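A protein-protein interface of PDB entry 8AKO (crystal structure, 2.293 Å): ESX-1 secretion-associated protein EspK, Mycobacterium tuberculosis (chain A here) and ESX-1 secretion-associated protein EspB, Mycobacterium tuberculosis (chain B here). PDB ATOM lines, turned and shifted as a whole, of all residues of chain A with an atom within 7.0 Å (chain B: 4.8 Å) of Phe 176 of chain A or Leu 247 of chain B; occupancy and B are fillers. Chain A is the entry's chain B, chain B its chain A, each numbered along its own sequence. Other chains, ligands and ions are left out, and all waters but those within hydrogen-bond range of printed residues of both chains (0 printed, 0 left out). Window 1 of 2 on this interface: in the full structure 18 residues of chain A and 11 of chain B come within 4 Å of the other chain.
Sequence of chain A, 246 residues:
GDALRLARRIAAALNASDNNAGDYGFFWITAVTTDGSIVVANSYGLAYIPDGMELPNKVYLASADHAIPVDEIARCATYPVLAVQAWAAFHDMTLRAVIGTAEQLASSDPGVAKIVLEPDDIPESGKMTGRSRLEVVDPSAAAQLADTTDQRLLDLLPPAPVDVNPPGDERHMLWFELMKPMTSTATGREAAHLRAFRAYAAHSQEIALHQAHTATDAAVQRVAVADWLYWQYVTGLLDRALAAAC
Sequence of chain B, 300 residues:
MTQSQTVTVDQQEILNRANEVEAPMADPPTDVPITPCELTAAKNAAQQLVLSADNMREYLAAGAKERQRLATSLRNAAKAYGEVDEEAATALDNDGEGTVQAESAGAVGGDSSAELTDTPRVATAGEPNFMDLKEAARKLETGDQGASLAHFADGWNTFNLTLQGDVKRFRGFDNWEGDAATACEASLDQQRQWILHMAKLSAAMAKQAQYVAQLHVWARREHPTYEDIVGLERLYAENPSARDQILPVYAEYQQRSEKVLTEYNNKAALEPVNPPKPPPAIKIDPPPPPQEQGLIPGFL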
ATOM      1  N   GLY A  22      17.929  30.991   5.517  1.00  0.00           N
ATOM      2  CA  GLY A  22      18.258  29.678   4.979  1.00  0.00           C
ATOM      3  C   GLY A  22      19.331  29.720   3.890  1.00  0.00           C
ATOM      4  O   GLY A  22      19.372  28.874   2.992  1.00  0.00           O
ATOM      5  N   ASP A  23      20.219  30.711   3.987  1.00  0.00           N
ATOM      6  CA  ASP A  23      21.327  30.830   3.053  1.00  0.00           C
ATOM      7  C   ASP A  23      22.467  29.931   3.522  1.00  0.00           C
ATOM      8  O   ASP A  23      23.066  30.168   4.572  1.00  0.00           O
ATOM      9  CB  ASP A  23      21.773  32.288   2.925  1.00  0.00           C
ATOM     10  CG  ASP A  23      20.776  33.156   2.174  1.00  0.00           C
ATOM     11  OD1 ASP A  23      20.337  32.737   1.078  1.00  0.00           O
ATOM     12  OD2 ASP A  23      20.443  34.247   2.690  1.00  0.00           O
ATOM     13  N   TYR A  24      22.743  28.891   2.726  1.00  0.00           N
ATOM     14  CA  TYR A  24      23.694  27.848   3.086  1.00  0.00           C
ATOM     15  C   TYR A  24      25.097  28.440   3.141  1.00  0.00           C
ATOM     16  O   TYR A  24      25.578  28.922   2.128  1.00  0.00           O
ATOM     17  CB  TYR A  24      23.633  26.688   2.076  1.00  0.00           C
ATOM     18  CG  TYR A  24      24.243  25.394   2.567  1.00  0.00           C
ATOM     19  CD1 TYR A  24      23.442  24.364   3.030  1.00  0.00           C
ATOM     20  CD2 TYR A  24      25.622  25.210   2.600  1.00  0.00           C
ATOM     21  CE1 TYR A  24      24.007  23.202   3.534  1.00  0.00           C
ATOM     22  CE2 TYR A  24      26.204  24.056   3.089  1.00  0.00           C
ATOM     23  CZ  TYR A  24      25.386  23.053   3.567  1.00  0.00           C
ATOM     24  OH  TYR A  24      25.961  21.917   4.044  1.00  0.00           O
ATOM     25  N   GLY A  25      25.744  28.406   4.308  1.00  0.00           N
ATOM     26  CA  GLY A  25      27.107  28.894   4.416  1.00  0.00           C
ATOM     27  C   GLY A  25      27.194  30.366   4.797  1.00  0.00           C
ATOM     28  O   GLY A  25      28.291  30.816   5.109  1.00  0.00           O
ATOM     29  N   TYR A  44      29.752  35.452   2.232  1.00  0.00           N
ATOM     30  CA  TYR A  44      29.358  35.448   0.833  1.00  0.00           C
ATOM     31  C   TYR A  44      30.087  36.550   0.073  1.00  0.00           C
ATOM     32  O   TYR A  44      29.672  37.703   0.078  1.00  0.00           O
ATOM     33  CB  TYR A  44      27.850  35.627   0.655  1.00  0.00           C
ATOM     34  CG  TYR A  44      27.063  34.350   0.737  1.00  0.00           C
ATOM     35  CD1 TYR A  44      27.674  33.179   1.145  1.00  0.00           C
ATOM     36  CD2 TYR A  44      25.724  34.312   0.390  1.00  0.00           C
ATOM     37  CE1 TYR A  44      26.967  31.995   1.221  1.00  0.00           C
ATOM     38  CE2 TYR A  44      24.999  33.139   0.476  1.00  0.00           C
ATOM     39  CZ  TYR A  44      25.622  31.976   0.895  1.00  0.00           C
ATOM     40  OH  TYR A  44      24.914  30.809   0.962  1.00  0.00           O
ATOM     41  N   ARG A 171      17.515  36.466 -11.008  1.00  0.00           N
ATOM     42  CA  ARG A 171      18.437  36.527  -9.885  1.00  0.00           C
ATOM     43  C   ARG A 171      18.257  35.332  -8.945  1.00  0.00           C
ATOM     44  O   ARG A 171      19.224  34.866  -8.346  1.00  0.00           O
ATOM     45  CB  ARG A 171      18.363  37.898  -9.197  1.00  0.00           C
ATOM     46  CG  ARG A 171      17.235  38.073  -8.192  1.00  0.00           C
ATOM     47  CD  ARG A 171      17.389  39.362  -7.408  1.00  0.00           C
ATOM     48  NE  ARG A 171      17.245  40.534  -8.265  1.00  0.00           N
ATOM     49  CZ  ARG A 171      16.896  41.740  -7.834  1.00  0.00           C
ATOM     50  NH1 ARG A 171      16.649  41.936  -6.547  1.00  0.00           N
ATOM     51  NH2 ARG A 171      16.793  42.740  -8.694  1.00  0.00           N
ATOM     52  N   HIS A 172      17.029  34.812  -8.858  1.00  0.00           N
ATOM     53  CA  HIS A 172      16.728  33.641  -8.048  1.00  0.00           C
ATOM     54  C   HIS A 172      17.455  32.405  -8.564  1.00  0.00           C
ATOM     55  O   HIS A 172      17.628  31.445  -7.820  1.00  0.00           O
ATOM     56  CB  HIS A 172      15.216  33.377  -8.008  1.00  0.00           C
ATOM     57  CG  HIS A 172      14.478  34.298  -7.100  1.00  0.00           C
ATOM     58  ND1 HIS A 172      14.893  34.538  -5.800  1.00  0.00           N
ATOM     59  CD2 HIS A 172      13.363  35.036  -7.289  1.00  0.00           C
ATOM     60  CE1 HIS A 172      14.064  35.387  -5.228  1.00  0.00           C
ATOM     61  NE2 HIS A 172      13.117  35.708  -6.121  1.00  0.00           N
ATOM     62  N   MET A 173      17.846  32.413  -9.844  1.00  0.00           N
ATOM     63  CA  MET A 173      18.693  31.347 -10.358  1.00  0.00           C
ATOM     64  C   MET A 173      20.157  31.601  -9.988  1.00  0.00           C
ATOM     65  O   MET A 173      20.829  30.696  -9.490  1.00  0.00           O
ATOM     66  CB  MET A 173      18.532  31.165 -11.877  1.00  0.00           C
ATOM     67  CG  MET A 173      17.204  30.526 -12.292  1.00  0.00           C
ATOM     68  SD  MET A 173      17.066  28.769 -11.842  1.00  0.00           S
ATOM     69  CE  MET A 173      16.199  28.777 -10.274  1.00  0.00           C
ATOM     70  N   LEU A 174      20.639  32.834 -10.210  1.00  0.00           N
ATOM     71  CA  LEU A 174      22.067  33.124 -10.131  1.00  0.00           C
ATOM     72  C   LEU A 174      22.539  33.032  -8.684  1.00  0.00           C
ATOM     73  O   LEU A 174      23.622  32.515  -8.421  1.00  0.00           O
ATOM     74  CB  LEU A 174      22.372  34.492 -10.748  1.00  0.00           C
ATOM     75  CG  LEU A 174      21.908  34.686 -12.192  1.00  0.00           C
ATOM     76  CD1 LEU A 174      22.454  35.982 -12.752  1.00  0.00           C
ATOM     77  CD2 LEU A 174      22.329  33.529 -13.085  1.00  0.00           C
ATOM     78  N   TRP A 175      21.669  33.473  -7.770  1.00  0.00           N
ATOM     79  CA  TRP A 175      21.817  33.282  -6.334  1.00  0.00           C
ATOM     80  C   TRP A 175      22.041  31.804  -5.997  1.00  0.00           C
ATOM     81  O   TRP A 175      22.990  31.471  -5.298  1.00  0.00           O
ATOM     82  CB  TRP A 175      20.610  33.865  -5.572  1.00  0.00           C
ATOM     83  CG  TRP A 175      20.823  33.915  -4.092  1.00  0.00           C
ATOM     84  CD1 TRP A 175      20.306  33.068  -3.159  1.00  0.00           C
ATOM     85  CD2 TRP A 175      21.636  34.858  -3.374  1.00  0.00           C
ATOM     86  NE1 TRP A 175      20.725  33.432  -1.905  1.00  0.00           N
ATOM     87  CE2 TRP A 175      21.564  34.511  -2.005  1.00  0.00           C
ATOM     88  CE3 TRP A 175      22.421  35.957  -3.750  1.00  0.00           C
ATOM     89  CZ2 TRP A 175      22.254  35.216  -1.012  1.00  0.00           C
ATOM     90  CZ3 TRP A 175      23.101  36.653  -2.766  1.00  0.00           C
ATOM     91  CH2 TRP A 175      23.017  36.287  -1.418  1.00  0.00           C
ATOM     92  N   PHE A 176      21.186  30.918  -6.530  1.00  0.00           N
ATOM     93  CA  PHE A 176      21.307  29.472  -6.360  1.00  0.00           C
ATOM     94  C   PHE A 176      22.672  28.968  -6.833  1.00  0.00           C
ATOM     95  O   PHE A 176      23.371  28.258  -6.102  1.00  0.00           O
ATOM     96  CB  PHE A 176      20.217  28.726  -7.143  1.00  0.00           C
ATOM     97  CG  PHE A 176      20.197  27.213  -6.998  1.00  0.00           C
ATOM     98  CD1 PHE A 176      19.880  26.409  -8.095  1.00  0.00           C
ATOM     99  CD2 PHE A 176      20.459  26.584  -5.771  1.00  0.00           C
ATOM    100  CE1 PHE A 176      19.821  25.027  -7.969  1.00  0.00           C
ATOM    101  CE2 PHE A 176      20.415  25.199  -5.646  1.00  0.00           C
ATOM    102  CZ  PHE A 176      20.082  24.428  -6.747  1.00  0.00           C
ATOM    103  N   GLU A 177      23.028  29.331  -8.070  1.00  0.00           N
ATOM    104  CA  GLU A 177      24.327  29.008  -8.648  1.00  0.00           C
ATOM    105  C   GLU A 177      25.451  29.408  -7.688  1.00  0.00           C
ATOM    106  O   GLU A 177      26.408  28.666  -7.471  1.00  0.00           O
ATOM    107  CB  GLU A 177      24.408  29.676 -10.023  1.00  0.00           C
ATOM    108  CG  GLU A 177      25.714  29.430 -10.736  1.00  0.00           C
ATOM    109  CD  GLU A 177      25.972  28.004 -11.195  1.00  0.00           C
ATOM    110  OE1 GLU A 177      24.987  27.301 -11.553  1.00  0.00           O
ATOM    111  OE2 GLU A 177      27.169  27.609 -11.204  1.00  0.00           O
ATOM    112  N   LEU A 178      25.300  30.596  -7.106  1.00  0.00           N
ATOM    113  CA  LEU A 178      26.188  31.188  -6.117  1.00  0.00           C
ATOM    114  C   LEU A 178      26.285  30.295  -4.879  1.00  0.00           C
ATOM    115  O   LEU A 178      27.353  30.214  -4.271  1.00  0.00           O
ATOM    116  CB  LEU A 178      25.551  32.541  -5.779  1.00  0.00           C
ATOM    117  CG  LEU A 178      26.164  33.592  -4.868  1.00  0.00           C
ATOM    118  CD1 LEU A 178      25.539  34.855  -5.391  1.00  0.00           C
ATOM    119  CD2 LEU A 178      25.734  33.428  -3.408  1.00  0.00           C
ATOM    120  N   MET A 179      25.185  29.633  -4.481  1.00  0.00           N
ATOM    121  CA  MET A 179      25.224  28.861  -3.241  1.00  0.00           C
ATOM    122  C   MET A 179      25.798  27.462  -3.469  1.00  0.00           C
ATOM    123  O   MET A 179      26.105  26.737  -2.518  1.00  0.00           O
ATOM    124  CB  MET A 179      23.833  28.716  -2.629  1.00  0.00           C
ATOM    125  CG  MET A 179      23.016  29.975  -2.761  1.00  0.00           C
ATOM    126  SD  MET A 179      21.418  29.923  -1.942  1.00  0.00           S
ATOM    127  CE  MET A 179      22.076  29.830  -0.280  1.00  0.00           C
ATOM    128  N   LYS A 180      25.962  27.080  -4.734  1.00  0.00           N
ATOM    129  CA  LYS A 180      26.421  25.731  -5.015  1.00  0.00           C
ATOM    130  C   LYS A 180      27.834  25.444  -4.486  1.00  0.00           C
ATOM    131  O   LYS A 180      27.989  24.398  -3.870  1.00  0.00           O
ATOM    132  CB  LYS A 180      26.225  25.382  -6.487  1.00  0.00           C
ATOM    133  CG  LYS A 180      24.789  25.127  -6.905  1.00  0.00           C
ATOM    134  CD  LYS A 180      24.695  25.057  -8.411  1.00  0.00           C
ATOM    135  CE  LYS A 180      23.299  24.720  -8.878  1.00  0.00           C
ATOM    136  NZ  LYS A 180      23.077  25.092 -10.296  1.00  0.00           N
ATOM    137  N   PRO A 181      28.920  26.253  -4.687  1.00  0.00           N
ATOM    138  CA  PRO A 181      30.206  25.891  -4.086  1.00  0.00           C
ATOM    139  C   PRO A 181      30.295  26.014  -2.575  1.00  0.00           C
ATOM    140  O   PRO A 181      31.275  25.548  -1.987  1.00  0.00           O
ATOM    141  CB  PRO A 181      31.217  26.835  -4.739  1.00  0.00           C
ATOM    142  CG  PRO A 181      30.504  27.333  -5.973  1.00  0.00           C
ATOM    143  CD  PRO A 181      29.059  27.436  -5.562  1.00  0.00           C
ATOM    144  N   THR A 183      28.465  24.550  -0.541  1.00  0.00           N
ATOM    145  CA  THR A 183      28.193  23.225  -0.012  1.00  0.00           C
ATOM    146  C   THR A 183      29.414  22.324  -0.124  1.00  0.00           C
ATOM    147  O   THR A 183      29.253  21.115  -0.051  1.00  0.00           O
ATOM    148  CB  THR A 183      27.062  22.563  -0.799  1.00  0.00           C
ATOM    149  OG1 THR A 183      27.538  22.223  -2.104  1.00  0.00           O
ATOM    150  CG2 THR A 183      25.853  23.465  -0.909  1.00  0.00           C
ATOM    151  N   ALA A 196      30.399  33.089  -9.605  1.00  0.00           N
ATOM    152  CA  ALA A 196      28.944  33.063  -9.659  1.00  0.00           C
ATOM    153  C   ALA A 196      28.370  34.339  -9.037  1.00  0.00           C
ATOM    154  O   ALA A 196      27.369  34.869  -9.529  1.00  0.00           O
ATOM    155  CB  ALA A 196      28.411  31.823  -8.984  1.00  0.00           C
ATOM    156  N   TYR A 200      26.021  37.383 -10.602  1.00  0.00           N
ATOM    157  CA  TYR A 200      24.881  37.910  -9.866  1.00  0.00           C
ATOM    158  C   TYR A 200      25.003  39.427  -9.733  1.00  0.00           C
ATOM    159  O   TYR A 200      24.012  40.149  -9.860  1.00  0.00           O
ATOM    160  CB  TYR A 200      24.774  37.249  -8.489  1.00  0.00           C
ATOM    161  CG  TYR A 200      23.665  37.780  -7.621  1.00  0.00           C
ATOM    162  CD1 TYR A 200      22.336  37.495  -7.903  1.00  0.00           C
ATOM    163  CD2 TYR A 200      23.942  38.560  -6.509  1.00  0.00           C
ATOM    164  CE1 TYR A 200      21.305  37.983  -7.111  1.00  0.00           C
ATOM    165  CE2 TYR A 200      22.922  39.052  -5.704  1.00  0.00           C
ATOM    166  CZ  TYR A 200      21.596  38.769  -6.007  1.00  0.00           C
ATOM    167  OH  TYR A 200      20.559  39.237  -5.244  1.00  0.00           O
ATOM    168  N   GLU B 233      17.716  20.692  -9.934  1.00  0.00           N
ATOM    169  CA  GLU B 233      17.888  22.076 -10.342  1.00  0.00           C
ATOM    170  C   GLU B 233      16.562  22.626 -10.850  1.00  0.00           C
ATOM    171  O   GLU B 233      16.188  23.748 -10.521  1.00  0.00           O
ATOM    172  CB  GLU B 233      18.976  22.188 -11.416  1.00  0.00           C
ATOM    173  CG  GLU B 233      20.391  22.113 -10.851  1.00  0.00           C
ATOM    174  CD  GLU B 233      21.477  22.150 -11.908  1.00  0.00           C
ATOM    175  OE1 GLU B 233      21.138  22.000 -13.109  1.00  0.00           O
ATOM    176  OE2 GLU B 233      22.654  22.325 -11.530  1.00  0.00           O
ATOM    177  N   TYR B 236      14.176  23.184  -7.875  1.00  0.00           N
ATOM    178  CA  TYR B 236      14.415  24.501  -7.297  1.00  0.00           C
ATOM    179  C   TYR B 236      13.828  25.590  -8.194  1.00  0.00           C
ATOM    180  O   TYR B 236      13.385  26.613  -7.686  1.00  0.00           O
ATOM    181  CB  TYR B 236      15.909  24.767  -7.103  1.00  0.00           C
ATOM    182  CG  TYR B 236      16.287  26.016  -6.335  1.00  0.00           C
ATOM    183  CD1 TYR B 236      16.733  25.941  -5.016  1.00  0.00           C
ATOM    184  CD2 TYR B 236      16.283  27.268  -6.935  1.00  0.00           C
ATOM    185  CE1 TYR B 236      17.150  27.064  -4.312  1.00  0.00           C
ATOM    186  CE2 TYR B 236      16.674  28.404  -6.237  1.00  0.00           C
ATOM    187  CZ  TYR B 236      17.115  28.307  -4.925  1.00  0.00           C
ATOM    188  OH  TYR B 236      17.527  29.430  -4.254  1.00  0.00           O
ATOM    189  N   ARG B 243      13.131  26.204  -1.475  1.00  0.00           N
ATOM    190  CA  ARG B 243      14.532  26.559  -1.577  1.00  0.00           C
ATOM    191  C   ARG B 243      15.253  26.340  -0.242  1.00  0.00           C
ATOM    192  O   ARG B 243      16.478  26.239  -0.226  1.00  0.00           O
ATOM    193  CB  ARG B 243      14.695  27.933  -2.248  1.00  0.00           C
ATOM    194  CG  ARG B 243      14.421  29.160  -1.382  1.00  0.00           C
ATOM    195  CD  ARG B 243      15.436  30.286  -1.571  1.00  0.00           C
ATOM    196  NE  ARG B 243      16.657  30.010  -0.810  1.00  0.00           N
ATOM    197  CZ  ARG B 243      17.477  30.916  -0.259  1.00  0.00           C
ATOM    198  NH1 ARG B 243      17.282  32.216  -0.434  1.00  0.00           N
ATOM    199  NH2 ARG B 243      18.521  30.506   0.441  1.00  0.00           N
ATOM    200  N   GLN B 245      14.875  23.690   1.662  1.00  0.00           N
ATOM    201  CA  GLN B 245      15.087  22.266   1.894  1.00  0.00           C
ATOM    202  C   GLN B 245      15.737  21.535   0.706  1.00  0.00           C
ATOM    203  O   GLN B 245      16.103  20.371   0.843  1.00  0.00           O
ATOM    204  CB  GLN B 245      13.820  21.585   2.419  1.00  0.00           C
ATOM    205  CG  GLN B 245      12.850  21.122   1.335  1.00  0.00           C
ATOM    206  CD  GLN B 245      11.704  20.333   1.925  1.00  0.00           C
ATOM    207  OE1 GLN B 245      11.430  20.411   3.125  1.00  0.00           O
ATOM    208  NE2 GLN B 245      11.026  19.562   1.088  1.00  0.00           N
ATOM    209  N   ILE B 246      15.904  22.201  -0.445  1.00  0.00           N
ATOM    210  CA  ILE B 246      16.614  21.634  -1.586  1.00  0.00           C
ATOM    211  C   ILE B 246      18.129  21.731  -1.369  1.00  0.00           C
ATOM    212  O   ILE B 246      18.890  20.865  -1.780  1.00  0.00           O
ATOM    213  CB  ILE B 246      16.088  22.285  -2.883  1.00  0.00           C
ATOM    214  CG1 ILE B 246      14.664  21.788  -3.123  1.00  0.00           C
ATOM    215  CG2 ILE B 246      16.966  22.032  -4.113  1.00  0.00           C
ATOM    216  CD1 ILE B 246      13.995  22.419  -4.296  1.00  0.00           C
ATOM    217  N   LEU B 247      18.559  22.732  -0.618  1.00  0.00           N
ATOM    218  CA  LEU B 247      19.968  22.937  -0.380  1.00  0.00           C
ATOM    219  C   LEU B 247      20.589  21.893   0.542  1.00  0.00           C
ATOM    220  O   LEU B 247      21.770  21.622   0.361  1.00  0.00           O
ATOM    221  CB  LEU B 247      20.182  24.338   0.183  1.00  0.00           C
ATOM    222  CG  LEU B 247      20.671  25.414  -0.785  1.00  0.00           C
ATOM    223  CD1 LEU B 247      19.826  25.519  -2.057  1.00  0.00           C
ATOM    224  CD2 LEU B 247      20.631  26.728  -0.038  1.00  0.00           C
ATOM    225  N   PRO B 248      19.960  21.329   1.605  1.00  0.00           N
ATOM    226  CA  PRO B 248      20.597  20.188   2.269  1.00  0.00           C
ATOM    227  C   PRO B 248      20.699  18.898   1.450  1.00  0.00           C
ATOM    228  O   PRO B 248      21.517  18.038   1.789  1.00  0.00           O
ATOM    229  CB  PRO B 248      19.793  19.993   3.552  1.00  0.00           C
ATOM    230  CG  PRO B 248      19.248  21.362   3.811  1.00  0.00           C
ATOM    231  CD  PRO B 248      18.851  21.848   2.421  1.00  0.00           C
ATOM    232  N   VAL B 249      19.917  18.762   0.368  1.00  0.00           N
ATOM    233  CA  VAL B 249      20.091  17.549  -0.422  1.00  0.00           C
ATOM    234  C   VAL B 249      21.294  17.695  -1.365  1.00  0.00           C
ATOM    235  O   VAL B 249      22.078  16.758  -1.540  1.00  0.00           O
ATOM    236  CB  VAL B 249      18.789  17.073  -1.105  1.00  0.00           C
ATOM    237  CG1 VAL B 249      17.588  17.139  -0.170  1.00  0.00           C
ATOM    238  CG2 VAL B 249      18.506  17.680  -2.479  1.00  0.00           C
ATOM    239  N   TYR B 250      21.468  18.909  -1.907  1.00  0.00           N
ATOM    240  CA  TYR B 250      22.504  19.221  -2.874  1.00  0.00           C
ATOM    241  C   TYR B 250      23.868  19.104  -2.210  1.00  0.00           C
ATOM    242  O   TYR B 250      24.765  18.557  -2.827  1.00  0.00           O
ATOM    243  CB  TYR B 250      22.307  20.623  -3.449  1.00  0.00           C
ATOM    244  CG  TYR B 250      23.117  20.949  -4.686  1.00  0.00           C
ATOM    245  CD1 TYR B 250      24.425  21.422  -4.621  1.00  0.00           C
ATOM    246  CD2 TYR B 250      22.547  20.854  -5.948  1.00  0.00           C
ATOM    247  CE1 TYR B 250      25.159  21.713  -5.775  1.00  0.00           C
ATOM    248  CE2 TYR B 250      23.255  21.170  -7.110  1.00  0.00           C
ATOM    249  CZ  TYR B 250      24.579  21.590  -7.032  1.00  0.00           C
ATOM    250  OH  TYR B 250      25.290  21.856  -8.183  1.00  0.00           O
ATOM    251  N   ALA B 251      23.990  19.594  -0.966  1.00  0.00           N
ATOM    252  CA  ALA B 251      25.204  19.428  -0.183  1.00  0.00           C
ATOM    253  C   ALA B 251      25.518  17.948   0.017  1.00  0.00           C
ATOM    254  O   ALA B 251      26.672  17.526  -0.105  1.00  0.00           O
ATOM    255  CB  ALA B 251      25.081  20.125   1.141  1.00  0.00           C
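The backbone carbonyl oxygen (O) of Gly 22 of chain A lies within hydrogen-bond range of the guanidinium group (NH2) of Arg 243 of chain B (3.1 Å). The side-chain amino group of Lys 180 of chain A is in salt-bridge range of the side-chain carboxylate of Glu 233 of chain B. The guanidinium group (NH2) of Arg 243 of chain B is in salt-bridge range of the side-chain carboxylate (OD1) of Asp 23 of chain A, at 2.9 Å. SD of Met 179 of chain A lies close to NH2 of Arg 243 of chain B, 3.8 Å away.
The backbone carbonyl oxygen (O) of Lys 180 of chain A is in hydrogen-bond range of the side-chain hydroxyl (OG1) of Thr 183 of chain A (2.8 Å). The backbone NH of Tyr 24 of chain A sits close to the side-chain hydroxyl of Tyr 44 of chain A. The side-chain carboxylate (OD1) of Asp 23 of chain A is in hydrogen-bond range of the indole nitrogen (NE1) of Trp 175 of chain A (3.1 Å). NZ of Lys 180 of chain A lies within salt-bridge range of OE1 of Glu 177 of chain A, at 3.2 Å. The indole nitrogen of Trp 175 of chain A sits close to the side-chain sulfur of Met 179 of chain A.
Among the printed residues, merely in contact across the chains: Lys 180 of chain A with Tyr 250 of chain B, Met 179 of chain A with Leu 247 of chain B, Tyr 24 of chain A with Ala 251 of chain B, His 172 of chain A with Tyr 236 of chain B, Phe 176 of chain A with Tyr 236 of chain B, Phe 176 of chain A with Leu 247 of chain B, Met 173 of chain A with Tyr 236 of chain B, Tyr 24 of chain A with Leu 247 of chain B, Thr 183 of chain A with Ala 251 of chain B, Gly 22 of chain A with Leu 247 of chain B and Trp 175 of chain A with Arg 243 of chain B.
Of the printed residues of chain B, Asp 23 of chain A touches Arg 243. Printed residues of chain B within 4 Å of His 172 of chain A: Tyr 236. Of the printed residues of chain B, Phe 176 of chain A touches Tyr 236 (3.6 Å) and Leu 247 (3.7 Å). Leu 178 of chain A touches none of the printed residues of chain B. Tyr 200 of chain A touches none of the printed residues of chain B. Printed residues of chain A within 4 Å of Glu 233 of chain B: Lys 180 (3.1 Å). Of chain A, only Gly 22 (3.9 Å), Tyr 24 (3.7 Å), Phe 176 (3.7 Å) and Met 179 (3.4 Å) come within 4 Å of Leu 247 of chain B. Printed residues of chain A within 4 Å of Ala 251 of chain B: Tyr 24 (3.5 Å) and Thr 183 (3.7 Å). The nearest residue of chain A that does not touch Leu 247 of chain B is Thr 183 of chain A (4.7 Å).
Hydrophobic or aromatic side chains of chain A within 4 Å of the printed part of chain B: Tyr 24, Met 173, Trp 175, Phe 176 and Met 179. Hydrophobic or aromatic side chains of chain B that line the printed part of chain A: Tyr 236, Leu 247, Tyr 250 and Ala 251. Among the printed residues, 15 pairs touch across the chains. Among the printed residues, Asp or Glu carboxylates within 4 Å of a Lys or Arg side-chain nitrogen of the other chain: Asp 23 of chain A with Arg 243 of chain B (2.9 Å) and Lys 180 of chain A with Glu 233 of chain B (3.1 Å).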
